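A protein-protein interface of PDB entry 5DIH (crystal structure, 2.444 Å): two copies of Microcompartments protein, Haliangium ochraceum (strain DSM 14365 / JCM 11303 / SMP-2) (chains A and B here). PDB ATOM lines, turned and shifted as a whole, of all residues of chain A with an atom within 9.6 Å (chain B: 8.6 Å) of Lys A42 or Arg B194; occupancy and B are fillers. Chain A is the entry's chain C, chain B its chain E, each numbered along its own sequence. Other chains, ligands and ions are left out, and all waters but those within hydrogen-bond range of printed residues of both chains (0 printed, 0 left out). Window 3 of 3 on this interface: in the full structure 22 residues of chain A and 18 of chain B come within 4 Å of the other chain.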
ATOM      1  N   ILE A  34     -16.532  11.195 -34.268  1.00  0.00           N
ATOM      2  CA  ILE A  34     -15.465  11.732 -33.436  1.00  0.00           C
ATOM      3  C   ILE A  34     -16.024  12.669 -32.365  1.00  0.00           C
ATOM      4  O   ILE A  34     -15.349  12.978 -31.382  1.00  0.00           O
ATOM      5  CB  ILE A  34     -14.421  12.480 -34.287  1.00  0.00           C
ATOM      6  CG1 ILE A  34     -13.044  12.421 -33.622  1.00  0.00           C
ATOM      7  CG2 ILE A  34     -14.862  13.911 -34.546  1.00  0.00           C
ATOM      8  CD1 ILE A  34     -12.462  11.026 -33.561  1.00  0.00           C
ATOM      9  N   THR A  35     -17.261  13.115 -32.558  1.00  0.00           N
ATOM     10  CA  THR A  35     -17.927  13.974 -31.586  1.00  0.00           C
ATOM     11  C   THR A  35     -18.545  13.118 -30.486  1.00  0.00           C
ATOM     12  O   THR A  35     -18.564  13.499 -29.316  1.00  0.00           O
ATOM     13  CB  THR A  35     -19.016  14.841 -32.245  1.00  0.00           C
ATOM     14  OG1 THR A  35     -18.470  15.512 -33.387  1.00  0.00           O
ATOM     15  CG2 THR A  35     -19.547  15.875 -31.262  1.00  0.00           C
ATOM     16  N   VAL A  36     -19.046  11.952 -30.880  1.00  0.00           N
ATOM     17  CA  VAL A  36     -19.605  10.992 -29.940  1.00  0.00           C
ATOM     18  C   VAL A  36     -18.521  10.464 -29.003  1.00  0.00           C
ATOM     19  O   VAL A  36     -18.747  10.303 -27.804  1.00  0.00           O
ATOM     20  CB  VAL A  36     -20.275   9.818 -30.681  1.00  0.00           C
ATOM     21  CG1 VAL A  36     -20.652   8.712 -29.711  1.00  0.00           C
ATOM     22  CG2 VAL A  36     -21.496  10.306 -31.445  1.00  0.00           C
ATOM     23  N   ALA A  37     -17.339  10.214 -29.557  1.00  0.00           N
ATOM     24  CA  ALA A  37     -16.214   9.706 -28.779  1.00  0.00           C
ATOM     25  C   ALA A  37     -15.746  10.723 -27.744  1.00  0.00           C
ATOM     26  O   ALA A  37     -15.302  10.357 -26.657  1.00  0.00           O
ATOM     27  CB  ALA A  37     -15.067   9.324 -29.698  1.00  0.00           C
ATOM     28  N   ASP A  38     -15.849  12.003 -28.087  1.00  0.00           N
ATOM     29  CA  ASP A  38     -15.438  13.065 -27.176  1.00  0.00           C
ATOM     30  C   ASP A  38     -16.449  13.251 -26.051  1.00  0.00           C
ATOM     31  O   ASP A  38     -16.087  13.610 -24.931  1.00  0.00           O
ATOM     32  CB  ASP A  38     -15.249  14.381 -27.933  1.00  0.00           C
ATOM     33  CG  ASP A  38     -14.868  15.528 -27.015  1.00  0.00           C
ATOM     34  OD1 ASP A  38     -13.688  15.602 -26.615  1.00  0.00           O
ATOM     35  OD2 ASP A  38     -15.748  16.356 -26.692  1.00  0.00           O
ATOM     36  N   ALA A  39     -17.719  13.006 -26.355  1.00  0.00           N
ATOM     37  CA  ALA A  39     -18.784  13.169 -25.373  1.00  0.00           C
ATOM     38  C   ALA A  39     -18.832  11.988 -24.412  1.00  0.00           C
ATOM     39  O   ALA A  39     -19.193  12.138 -23.244  1.00  0.00           O
ATOM     40  CB  ALA A  39     -20.124  13.338 -26.069  1.00  0.00           C
ATOM     41  N   ALA A  40     -18.461  10.815 -24.910  1.00  0.00           N
ATOM     42  CA  ALA A  40     -18.502   9.600 -24.105  1.00  0.00           C
ATOM     43  C   ALA A  40     -17.412   9.595 -23.037  1.00  0.00           C
ATOM     44  O   ALA A  40     -17.591   9.027 -21.959  1.00  0.00           O
ATOM     45  CB  ALA A  40     -18.376   8.374 -24.997  1.00  0.00           C
ATOM     46  N   LEU A  41     -16.286  10.235 -23.338  1.00  0.00           N
ATOM     47  CA  LEU A  41     -15.143  10.237 -22.430  1.00  0.00           C
ATOM     48  C   LEU A  41     -15.193  11.386 -21.427  1.00  0.00           C
ATOM     49  O   LEU A  41     -14.528  11.344 -20.389  1.00  0.00           O
ATOM     50  CB  LEU A  41     -13.838  10.294 -23.227  1.00  0.00           C
ATOM     51  CG  LEU A  41     -13.530   9.029 -24.028  1.00  0.00           C
ATOM     52  CD1 LEU A  41     -12.246   9.180 -24.825  1.00  0.00           C
ATOM     53  CD2 LEU A  41     -13.447   7.831 -23.098  1.00  0.00           C
ATOM     54  N   LYS A  42     -15.985  12.408 -21.731  1.00  0.00           N
ATOM     55  CA  LYS A  42     -16.091  13.570 -20.856  1.00  0.00           C
ATOM     56  C   LYS A  42     -17.154  13.382 -19.781  1.00  0.00           C
ATOM     57  O   LYS A  42     -17.285  14.207 -18.877  1.00  0.00           O
ATOM     58  CB  LYS A  42     -16.389  14.828 -21.672  1.00  0.00           C
ATOM     59  CG  LYS A  42     -15.162  15.428 -22.334  1.00  0.00           C
ATOM     60  CD  LYS A  42     -15.533  16.557 -23.272  1.00  0.00           C
ATOM     61  CE  LYS A  42     -14.291  17.176 -23.893  1.00  0.00           C
ATOM     62  NZ  LYS A  42     -14.619  18.035 -25.063  1.00  0.00           N
ATOM     63  N   ARG A  43     -17.875  12.272 -19.889  1.00  0.00           N
ATOM     64  CA  ARG A  43     -18.918  11.952 -18.955  1.00  0.00           C
ATOM     65  C   ARG A  43     -18.601  10.719 -18.173  1.00  0.00           C
ATOM     66  O   ARG A  43     -19.196  10.474 -17.157  1.00  0.00           O
ATOM     67  CB  ARG A  43     -20.272  11.924 -19.629  1.00  0.00           C
ATOM     68  CG  ARG A  43     -20.717  13.330 -19.966  1.00  0.00           C
ATOM     69  CD  ARG A  43     -22.195  13.497 -20.243  1.00  0.00           C
ATOM     70  NE  ARG A  43     -22.993  12.553 -19.509  1.00  0.00           N
ATOM     71  CZ  ARG A  43     -24.256  12.293 -19.779  1.00  0.00           C
ATOM     72  NH1 ARG A  43     -24.851  12.933 -20.763  1.00  0.00           N
ATOM     73  NH2 ARG A  43     -24.916  11.422 -19.047  1.00  0.00           N
ATOM     74  N   ALA A  44     -17.636   9.964 -18.637  1.00  0.00           N
ATOM     75  CA  ALA A  44     -17.161   8.755 -17.970  1.00  0.00           C
ATOM     76  C   ALA A  44     -15.789   8.353 -18.506  1.00  0.00           C
ATOM     77  O   ALA A  44     -15.552   8.410 -19.712  1.00  0.00           O
ATOM     78  CB  ALA A  44     -18.158   7.621 -18.142  1.00  0.00           C
ATOM     79  N   PRO A  45     -14.880   7.948 -17.605  1.00  0.00           N
ATOM     80  CA  PRO A  45     -13.489   7.633 -17.955  1.00  0.00           C
ATOM     81  C   PRO A  45     -13.288   6.222 -18.511  1.00  0.00           C
ATOM     82  O   PRO A  45     -12.587   5.417 -17.896  1.00  0.00           O
ATOM     83  CB  PRO A  45     -12.761   7.789 -16.622  1.00  0.00           C
ATOM     84  CG  PRO A  45     -13.784   7.397 -15.610  1.00  0.00           C
ATOM     85  CD  PRO A  45     -15.115   7.853 -16.152  1.00  0.00           C
ATOM     86  N   SER A  46     -13.886   5.931 -19.662  1.00  0.00           N
ATOM     87  CA  SER A  46     -13.687   4.643 -20.315  1.00  0.00           C
ATOM     88  C   SER A  46     -12.384   4.642 -21.109  1.00  0.00           C
ATOM     89  O   SER A  46     -11.786   5.692 -21.340  1.00  0.00           O
ATOM     90  CB  SER A  46     -14.866   4.312 -21.233  1.00  0.00           C
ATOM     91  OG  SER A  46     -16.083   4.251 -20.511  1.00  0.00           O
ATOM     92  N   MET A  63     -15.205   1.090 -26.979  1.00  0.00           N
ATOM     93  CA  MET A  63     -14.711   1.558 -25.693  1.00  0.00           C
ATOM     94  C   MET A  63     -14.659   0.421 -24.683  1.00  0.00           C
ATOM     95  O   MET A  63     -15.339  -0.594 -24.836  1.00  0.00           O
ATOM     96  CB  MET A  63     -15.582   2.699 -25.161  1.00  0.00           C
ATOM     97  CG  MET A  63     -17.039   2.328 -24.957  1.00  0.00           C
ATOM     98  SD  MET A  63     -18.036   3.735 -24.432  1.00  0.00           S
ATOM     99  CE  MET A  63     -17.687   4.897 -25.749  1.00  0.00           C
ATOM    100  N   GLU A  69     -18.916   2.478 -16.028  1.00  0.00           N
ATOM    101  CA  GLU A  69     -18.186   3.422 -16.871  1.00  0.00           C
ATOM    102  C   GLU A  69     -18.718   3.422 -18.299  1.00  0.00           C
ATOM    103  O   GLU A  69     -18.969   4.478 -18.877  1.00  0.00           O
ATOM    104  CB  GLU A  69     -16.691   3.095 -16.878  1.00  0.00           C
ATOM    105  CG  GLU A  69     -15.955   3.495 -15.612  1.00  0.00           C
ATOM    106  CD  GLU A  69     -14.474   3.177 -15.677  1.00  0.00           C
ATOM    107  OE1 GLU A  69     -14.088   2.302 -16.481  1.00  0.00           O
ATOM    108  OE2 GLU A  69     -13.695   3.804 -14.929  1.00  0.00           O
ATOM    109  N   GLU A  72     -22.484   4.631 -18.568  1.00  0.00           N
ATOM    110  CA  GLU A  72     -22.604   6.083 -18.491  1.00  0.00           C
ATOM    111  C   GLU A  72     -22.100   6.757 -19.768  1.00  0.00           C
ATOM    112  O   GLU A  72     -22.612   7.803 -20.167  1.00  0.00           O
ATOM    113  CB  GLU A  72     -21.838   6.617 -17.279  1.00  0.00           C
ATOM    114  CG  GLU A  72     -22.226   8.030 -16.861  1.00  0.00           C
ATOM    115  CD  GLU A  72     -23.573   8.087 -16.159  1.00  0.00           C
ATOM    116  OE1 GLU A  72     -24.069   7.024 -15.726  1.00  0.00           O
ATOM    117  OE2 GLU A  72     -24.137   9.195 -16.039  1.00  0.00           O
ATOM    118  N   SER A  73     -21.100   6.153 -20.404  1.00  0.00           N
ATOM    119  CA  SER A  73     -20.528   6.698 -21.634  1.00  0.00           C
ATOM    120  C   SER A  73     -21.476   6.553 -22.817  1.00  0.00           C
ATOM    121  O   SER A  73     -21.555   7.436 -23.671  1.00  0.00           O
ATOM    122  CB  SER A  73     -19.199   6.014 -21.962  1.00  0.00           C
ATOM    123  OG  SER A  73     -18.176   6.413 -21.070  1.00  0.00           O
ATOM    124  N   MET A  74     -22.190   5.432 -22.864  1.00  0.00           N
ATOM    125  CA  MET A  74     -23.093   5.142 -23.973  1.00  0.00           C
ATOM    126  C   MET A  74     -24.339   6.021 -23.930  1.00  0.00           C
ATOM    127  O   MET A  74     -24.977   6.258 -24.956  1.00  0.00           O
ATOM    128  CB  MET A  74     -23.488   3.664 -23.960  1.00  0.00           C
ATOM    129  CG  MET A  74     -22.308   2.713 -24.088  1.00  0.00           C
ATOM    130  SD  MET A  74     -21.483   2.818 -25.686  1.00  0.00           S
ATOM    131  CE  MET A  74     -22.696   2.019 -26.733  1.00  0.00           C
ATOM    132  N   ALA A  76     -24.314   9.284 -22.965  1.00  0.00           N
ATOM    133  CA  ALA A  76     -23.862  10.517 -23.598  1.00  0.00           C
ATOM    134  C   ALA A  76     -23.663  10.305 -25.094  1.00  0.00           C
ATOM    135  O   ALA A  76     -23.784  11.238 -25.888  1.00  0.00           O
ATOM    136  CB  ALA A  76     -22.574  11.007 -22.955  1.00  0.00           C
ATOM    137  N   ALA A  77     -23.355   9.069 -25.468  1.00  0.00           N
ATOM    138  CA  ALA A  77     -23.157   8.713 -26.865  1.00  0.00           C
ATOM    139  C   ALA A  77     -24.469   8.780 -27.641  1.00  0.00           C
ATOM    140  O   ALA A  77     -24.546   9.415 -28.691  1.00  0.00           O
ATOM    141  CB  ALA A  77     -22.548   7.327 -26.973  1.00  0.00           C
ATOM    142  N   ILE A  80     -25.759  12.295 -28.531  1.00  0.00           N
ATOM    143  CA  ILE A  80     -25.095  12.984 -29.633  1.00  0.00           C
ATOM    144  C   ILE A  80     -25.317  12.254 -30.956  1.00  0.00           C
ATOM    145  O   ILE A  80     -25.439  12.881 -32.008  1.00  0.00           O
ATOM    146  CB  ILE A  80     -23.580  13.126 -29.375  1.00  0.00           C
ATOM    147  CG1 ILE A  80     -23.329  13.702 -27.980  1.00  0.00           C
ATOM    148  CG2 ILE A  80     -22.929  14.001 -30.435  1.00  0.00           C
ATOM    149  CD1 ILE A  80     -23.940  15.069 -27.765  1.00  0.00           C
ATOM    150  N   TRP B 114      -0.311  16.114 -31.833  1.00  0.00           N
ATOM    151  CA  TRP B 114      -0.587  17.539 -31.972  1.00  0.00           C
ATOM    152  C   TRP B 114       0.052  18.342 -30.842  1.00  0.00           C
ATOM    153  O   TRP B 114       1.129  18.916 -31.006  1.00  0.00           O
ATOM    154  CB  TRP B 114      -2.097  17.789 -32.007  1.00  0.00           C
ATOM    155  CG  TRP B 114      -2.795  17.086 -33.132  1.00  0.00           C
ATOM    156  CD1 TRP B 114      -2.230  16.622 -34.285  1.00  0.00           C
ATOM    157  CD2 TRP B 114      -4.188  16.755 -33.208  1.00  0.00           C
ATOM    158  NE1 TRP B 114      -3.184  16.030 -35.076  1.00  0.00           N
ATOM    159  CE2 TRP B 114      -4.394  16.097 -34.437  1.00  0.00           C
ATOM    160  CE3 TRP B 114      -5.279  16.953 -32.356  1.00  0.00           C
ATOM    161  CZ2 TRP B 114      -5.647  15.637 -34.836  1.00  0.00           C
ATOM    162  CZ3 TRP B 114      -6.524  16.495 -32.755  1.00  0.00           C
ATOM    163  CH2 TRP B 114      -6.697  15.845 -33.983  1.00  0.00           C
ATOM    164  N   GLU B 119      -4.808  21.518 -30.177  1.00  0.00           N
ATOM    165  CA  GLU B 119      -5.780  22.167 -29.306  1.00  0.00           C
ATOM    166  C   GLU B 119      -7.188  22.026 -29.879  1.00  0.00           C
ATOM    167  O   GLU B 119      -7.820  20.979 -29.737  1.00  0.00           O
ATOM    168  CB  GLU B 119      -5.425  23.644 -29.111  1.00  0.00           C
ATOM    169  CG  GLU B 119      -6.123  24.318 -27.935  1.00  0.00           C
ATOM    170  CD  GLU B 119      -5.537  23.923 -26.591  1.00  0.00           C
ATOM    171  OE1 GLU B 119      -4.524  23.191 -26.566  1.00  0.00           O
ATOM    172  OE2 GLU B 119      -6.090  24.349 -25.557  1.00  0.00           O
ATOM    173  N   SER B 120      -7.673  23.079 -30.529  1.00  0.00           N
ATOM    174  CA  SER B 120      -8.992  23.054 -31.153  1.00  0.00           C
ATOM    175  C   SER B 120      -8.918  22.407 -32.530  1.00  0.00           C
ATOM    176  O   SER B 120      -7.884  22.466 -33.194  1.00  0.00           O
ATOM    177  CB  SER B 120      -9.564  24.469 -31.261  1.00  0.00           C
ATOM    178  OG  SER B 120      -9.612  25.096 -29.991  1.00  0.00           O
ATOM    179  N   VAL B 121     -10.015  21.791 -32.961  1.00  0.00           N
ATOM    180  CA  VAL B 121     -10.015  21.072 -34.228  1.00  0.00           C
ATOM    181  C   VAL B 121     -11.410  21.003 -34.856  1.00  0.00           C
ATOM    182  O   VAL B 121     -12.419  20.917 -34.153  1.00  0.00           O
ATOM    183  CB  VAL B 121      -9.451  19.637 -34.042  1.00  0.00           C
ATOM    184  CG1 VAL B 121     -10.345  18.816 -33.119  1.00  0.00           C
ATOM    185  CG2 VAL B 121      -9.263  18.939 -35.382  1.00  0.00           C
ATOM    186  N   GLY B 166      -5.752  24.441 -34.621  1.00  0.00           N
ATOM    187  CA  GLY B 166      -5.273  25.786 -34.366  1.00  0.00           C
ATOM    188  C   GLY B 166      -6.039  26.425 -33.231  1.00  0.00           C
ATOM    189  O   GLY B 166      -6.743  25.741 -32.491  1.00  0.00           O
ATOM    190  N   GLU B 167      -5.896  27.741 -33.094  1.00  0.00           N
ATOM    191  CA  GLU B 167      -6.635  28.503 -32.089  1.00  0.00           C
ATOM    192  C   GLU B 167      -8.138  28.352 -32.301  1.00  0.00           C
ATOM    193  O   GLU B 167      -8.581  28.041 -33.407  1.00  0.00           O
ATOM    194  CB  GLU B 167      -6.244  29.984 -32.129  1.00  0.00           C
ATOM    195  CG  GLU B 167      -4.787  30.264 -31.774  1.00  0.00           C
ATOM    196  CD  GLU B 167      -4.563  30.425 -30.281  1.00  0.00           C
ATOM    197  OE1 GLU B 167      -5.447  30.029 -29.493  1.00  0.00           O
ATOM    198  OE2 GLU B 167      -3.501  30.958 -29.894  1.00  0.00           O
ATOM    199  N   LEU B 168      -8.912  28.569 -31.243  1.00  0.00           N
ATOM    200  CA  LEU B 168     -10.357  28.371 -31.293  1.00  0.00           C
ATOM    201  C   LEU B 168     -11.018  29.258 -32.345  1.00  0.00           C
ATOM    202  O   LEU B 168     -11.747  28.767 -33.207  1.00  0.00           O
ATOM    203  CB  LEU B 168     -10.975  28.634 -29.921  1.00  0.00           C
ATOM    204  CG  LEU B 168     -12.472  28.356 -29.792  1.00  0.00           C
ATOM    205  CD1 LEU B 168     -12.787  26.928 -30.207  1.00  0.00           C
ATOM    206  CD2 LEU B 168     -12.939  28.616 -28.371  1.00  0.00           C
ATOM    207  N   VAL B 171     -10.283  28.215 -35.910  1.00  0.00           N
ATOM    208  CA  VAL B 171     -11.003  26.987 -36.229  1.00  0.00           C
ATOM    209  C   VAL B 171     -12.471  27.290 -36.532  1.00  0.00           C
ATOM    210  O   VAL B 171     -13.054  26.724 -37.459  1.00  0.00           O
ATOM    211  CB  VAL B 171     -10.892  25.962 -35.073  1.00  0.00           C
ATOM    212  CG1 VAL B 171     -11.969  24.903 -35.175  1.00  0.00           C
ATOM    213  CG2 VAL B 171      -9.510  25.321 -35.060  1.00  0.00           C
ATOM    214  N   GLU B 172     -13.058  28.200 -35.760  1.00  0.00           N
ATOM    215  CA  GLU B 172     -14.433  28.637 -35.993  1.00  0.00           C
ATOM    216  C   GLU B 172     -14.550  29.384 -37.321  1.00  0.00           C
ATOM    217  O   GLU B 172     -15.514  29.201 -38.065  1.00  0.00           O
ATOM    218  CB  GLU B 172     -14.923  29.532 -34.849  1.00  0.00           C
ATOM    219  CG  GLU B 172     -14.834  28.912 -33.458  1.00  0.00           C
ATOM    220  CD  GLU B 172     -15.859  27.819 -33.222  1.00  0.00           C
ATOM    221  OE1 GLU B 172     -16.861  27.764 -33.965  1.00  0.00           O
ATOM    222  OE2 GLU B 172     -15.662  27.014 -32.286  1.00  0.00           O
ATOM    223  N   CYS B 191     -17.088  20.569 -34.808  1.00  0.00           N
ATOM    224  CA  CYS B 191     -16.152  21.514 -34.214  1.00  0.00           C
ATOM    225  C   CYS B 191     -15.973  21.260 -32.721  1.00  0.00           C
ATOM    226  O   CYS B 191     -16.911  21.413 -31.938  1.00  0.00           O
ATOM    227  CB  CYS B 191     -16.626  22.948 -34.453  1.00  0.00           C
ATOM    228  SG  CYS B 191     -15.411  24.213 -34.031  1.00  0.00           S
ATOM    229  N   ILE B 192     -14.764  20.869 -32.332  1.00  0.00           N
ATOM    230  CA  ILE B 192     -14.460  20.607 -30.929  1.00  0.00           C
ATOM    231  C   ILE B 192     -13.439  21.610 -30.401  1.00  0.00           C
ATOM    232  O   ILE B 192     -12.337  21.726 -30.936  1.00  0.00           O
ATOM    233  CB  ILE B 192     -13.925  19.178 -30.723  1.00  0.00           C
ATOM    234  CG1 ILE B 192     -14.888  18.156 -31.331  1.00  0.00           C
ATOM    235  CG2 ILE B 192     -13.710  18.897 -29.241  1.00  0.00           C
ATOM    236  CD1 ILE B 192     -14.465  16.719 -31.121  1.00  0.00           C
ATOM    237  N   ALA B 193     -13.816  22.332 -29.349  1.00  0.00           N
ATOM    238  CA  ALA B 193     -12.960  23.361 -28.770  1.00  0.00           C
ATOM    239  C   ALA B 193     -11.706  22.761 -28.140  1.00  0.00           C
ATOM    240  O   ALA B 193     -10.597  23.246 -28.361  1.00  0.00           O
ATOM    241  CB  ALA B 193     -13.732  24.171 -27.741  1.00  0.00           C
ATOM    242  N   ARG B 194     -11.891  21.710 -27.350  1.00  0.00           N
ATOM    243  CA  ARG B 194     -10.772  21.007 -26.734  1.00  0.00           C
ATOM    244  C   ARG B 194     -11.138  19.556 -26.451  1.00  0.00           C
ATOM    245  O   ARG B 194     -11.793  19.257 -25.450  1.00  0.00           O
ATOM    246  CB  ARG B 194     -10.333  21.704 -25.443  1.00  0.00           C
ATOM    247  CG  ARG B 194      -9.219  20.979 -24.701  1.00  0.00           C
ATOM    248  CD  ARG B 194      -8.868  21.667 -23.391  1.00  0.00           C
ATOM    249  NE  ARG B 194      -8.121  22.904 -23.599  1.00  0.00           N
ATOM    250  CZ  ARG B 194      -7.692  23.691 -22.618  1.00  0.00           C
ATOM    251  NH1 ARG B 194      -7.938  23.373 -21.354  1.00  0.00           N
ATOM    252  NH2 ARG B 194      -7.016  24.796 -22.901  1.00  0.00           N
ATOM    253  N   PRO B 195     -10.722  18.646 -27.341  1.00  0.00           N
ATOM    254  CA  PRO B 195     -10.972  17.213 -27.169  1.00  0.00           C
ATOM    255  C   PRO B 195     -10.196  16.624 -25.995  1.00  0.00           C
ATOM    256  O   PRO B 195      -9.255  17.246 -25.501  1.00  0.00           O
ATOM    257  CB  PRO B 195     -10.497  16.611 -28.496  1.00  0.00           C
ATOM    258  CG  PRO B 195      -9.510  17.595 -29.024  1.00  0.00           C
ATOM    259  CD  PRO B 195     -10.029  18.936 -28.608  1.00  0.00           C
ATOM    260  N   VAL B 196     -10.595  15.433 -25.561  1.00  0.00           N
ATOM    261  CA  VAL B 196      -9.935  14.755 -24.452  1.00  0.00           C
ATOM    262  C   VAL B 196      -8.495  14.388 -24.799  1.00  0.00           C
ATOM    263  O   VAL B 196      -8.092  14.446 -25.961  1.00  0.00           O
ATOM    264  CB  VAL B 196     -10.696  13.483 -24.047  1.00  0.00           C
ATOM    265  CG1 VAL B 196     -12.098  13.835 -23.580  1.00  0.00           C
ATOM    266  CG2 VAL B 196     -10.752  12.511 -25.211  1.00  0.00           C
ATOM    267  N   ASP B 197      -7.723  14.006 -23.785  1.00  0.00           N
ATOM    268  CA  ASP B 197      -6.320  13.653 -23.981  1.00  0.00           C
ATOM    269  C   ASP B 197      -6.159  12.360 -24.775  1.00  0.00           C
ATOM    270  O   ASP B 197      -5.113  12.116 -25.373  1.00  0.00           O
ATOM    271  CB  ASP B 197      -5.608  13.524 -22.633  1.00  0.00           C
ATOM    272  CG  ASP B 197      -5.452  14.854 -21.929  1.00  0.00           C
ATOM    273  OD1 ASP B 197      -4.597  15.657 -22.361  1.00  0.00           O
ATOM    274  OD2 ASP B 197      -6.181  15.099 -20.944  1.00  0.00           O
ATOM    275  N   LEU B 199      -7.829  11.779 -27.297  1.00  0.00           N
ATOM    276  CA  LEU B 199      -8.191  12.178 -28.653  1.00  0.00           C
ATOM    277  C   LEU B 199      -7.185  13.180 -29.210  1.00  0.00           C
ATOM    278  O   LEU B 199      -6.979  13.260 -30.422  1.00  0.00           O
ATOM    279  CB  LEU B 199      -9.598  12.777 -28.681  1.00  0.00           C
ATOM    280  CG  LEU B 199     -10.682  11.957 -29.381  1.00  0.00           C
ATOM    281  CD1 LEU B 199     -10.665  10.530 -28.879  1.00  0.00           C
ATOM    282  CD2 LEU B 199     -12.052  12.583 -29.164  1.00  0.00           C
ATOM    283  N   ARG B 200      -6.566  13.945 -28.317  1.00  0.00           N
ATOM    284  CA  ARG B 200      -5.573  14.935 -28.716  1.00  0.00           C
ATOM    285  C   ARG B 200      -4.316  14.253 -29.241  1.00  0.00           C
ATOM    286  O   ARG B 200      -3.632  13.542 -28.506  1.00  0.00           O
ATOM    287  CB  ARG B 200      -5.221  15.851 -27.546  1.00  0.00           C
ATOM    288  CG  ARG B 200      -5.226  17.329 -27.893  1.00  0.00           C
ATOM    289  CD  ARG B 200      -4.533  18.149 -26.816  1.00  0.00           C
ATOM    290  NE  ARG B 200      -4.802  17.632 -25.478  1.00  0.00           N
ATOM    291  CZ  ARG B 200      -5.871  17.947 -24.753  1.00  0.00           C
ATOM    292  NH1 ARG B 200      -6.782  18.779 -25.236  1.00  0.00           N
ATOM    293  NH2 ARG B 200      -6.031  17.426 -23.545  1.00  0.00           N
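Among the printed residues, pairs that only touch across the chains: Asp A38 with Pro B195, Leu A41 with Val B196, Lys A42 with Val B196, Ile A34 with Ile B192, Asp A38 with Leu B199 and Ile A34 with Leu B199.
Hydrophobic or aromatic side chains of chain B within 4 Å of the printed part of chain A: Ile B192, Pro B195, Val B196 and Leu B199. Of the 21 printed residues of chain A, 4 touch a printed residue of chain B. Hydrophobic or aromatic side chains of chain A that line the printed part of chain B: Leu A41. Among the printed residues, 8 pairs touch across the chains. Among the printed residues, no Asp or Glu carboxylate lies within 4 Å of a Lys or Arg side-chain nitrogen of the other chain.
Printed residues of chain B within 4 Å of Ile A34: Ile B192 and Leu B199. Printed residues of chain B within 4 Å of Asp A38: Pro B195, Val B196 and Leu B199. Of the printed residues of chain B, Lys A42 touches Arg B194 and Val B196. Ser A46 touches none of the printed residues of chain B. Ala A77 touches none of the printed residues of chain B. No residue of chain A comes within 4 Å of Ala B193. Of chain A, only Lys A42 (3.1 Å) comes within 4 Å of Arg B194. Printed residues of chain A within 4 Å of Leu B199: Ile A34 (3.99 Å) and Asp A38 (3.9 Å). The nearest residue of chain A that does not touch Arg B194 is Asp A38 (4.3 Å). The nearest printed residue of chain A that does not touch Val B196 is Ala A37 (5.2 Å).
The backbone carbonyl oxygen of Arg B194 lies within hydrogen-bond range of the side-chain amino group of Lys A42. The side-chain carboxylate of Asp A38 lies within hydrogen-bond range of the backbone NH of Val B196, 3.3 Å away.
The backbone carbonyl oxygen of Val B121 lies within hydrogen-bond range of the backbone NH of Ile B192, 3.0 Å away. OD2 of Asp A38 lies within salt-bridge range of NZ of Lys A42, 2.6 Å away. The backbone carbonyl oxygen (O) of Pro B195 sits at hydrogen-bond distance from the guanidinium group (NH1) of Arg B200 (2.9 Å). NH2 of Arg B194 is in salt-bridge range of OE2 of Glu B119 (2.8 Å).
No position is printed for both chains.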
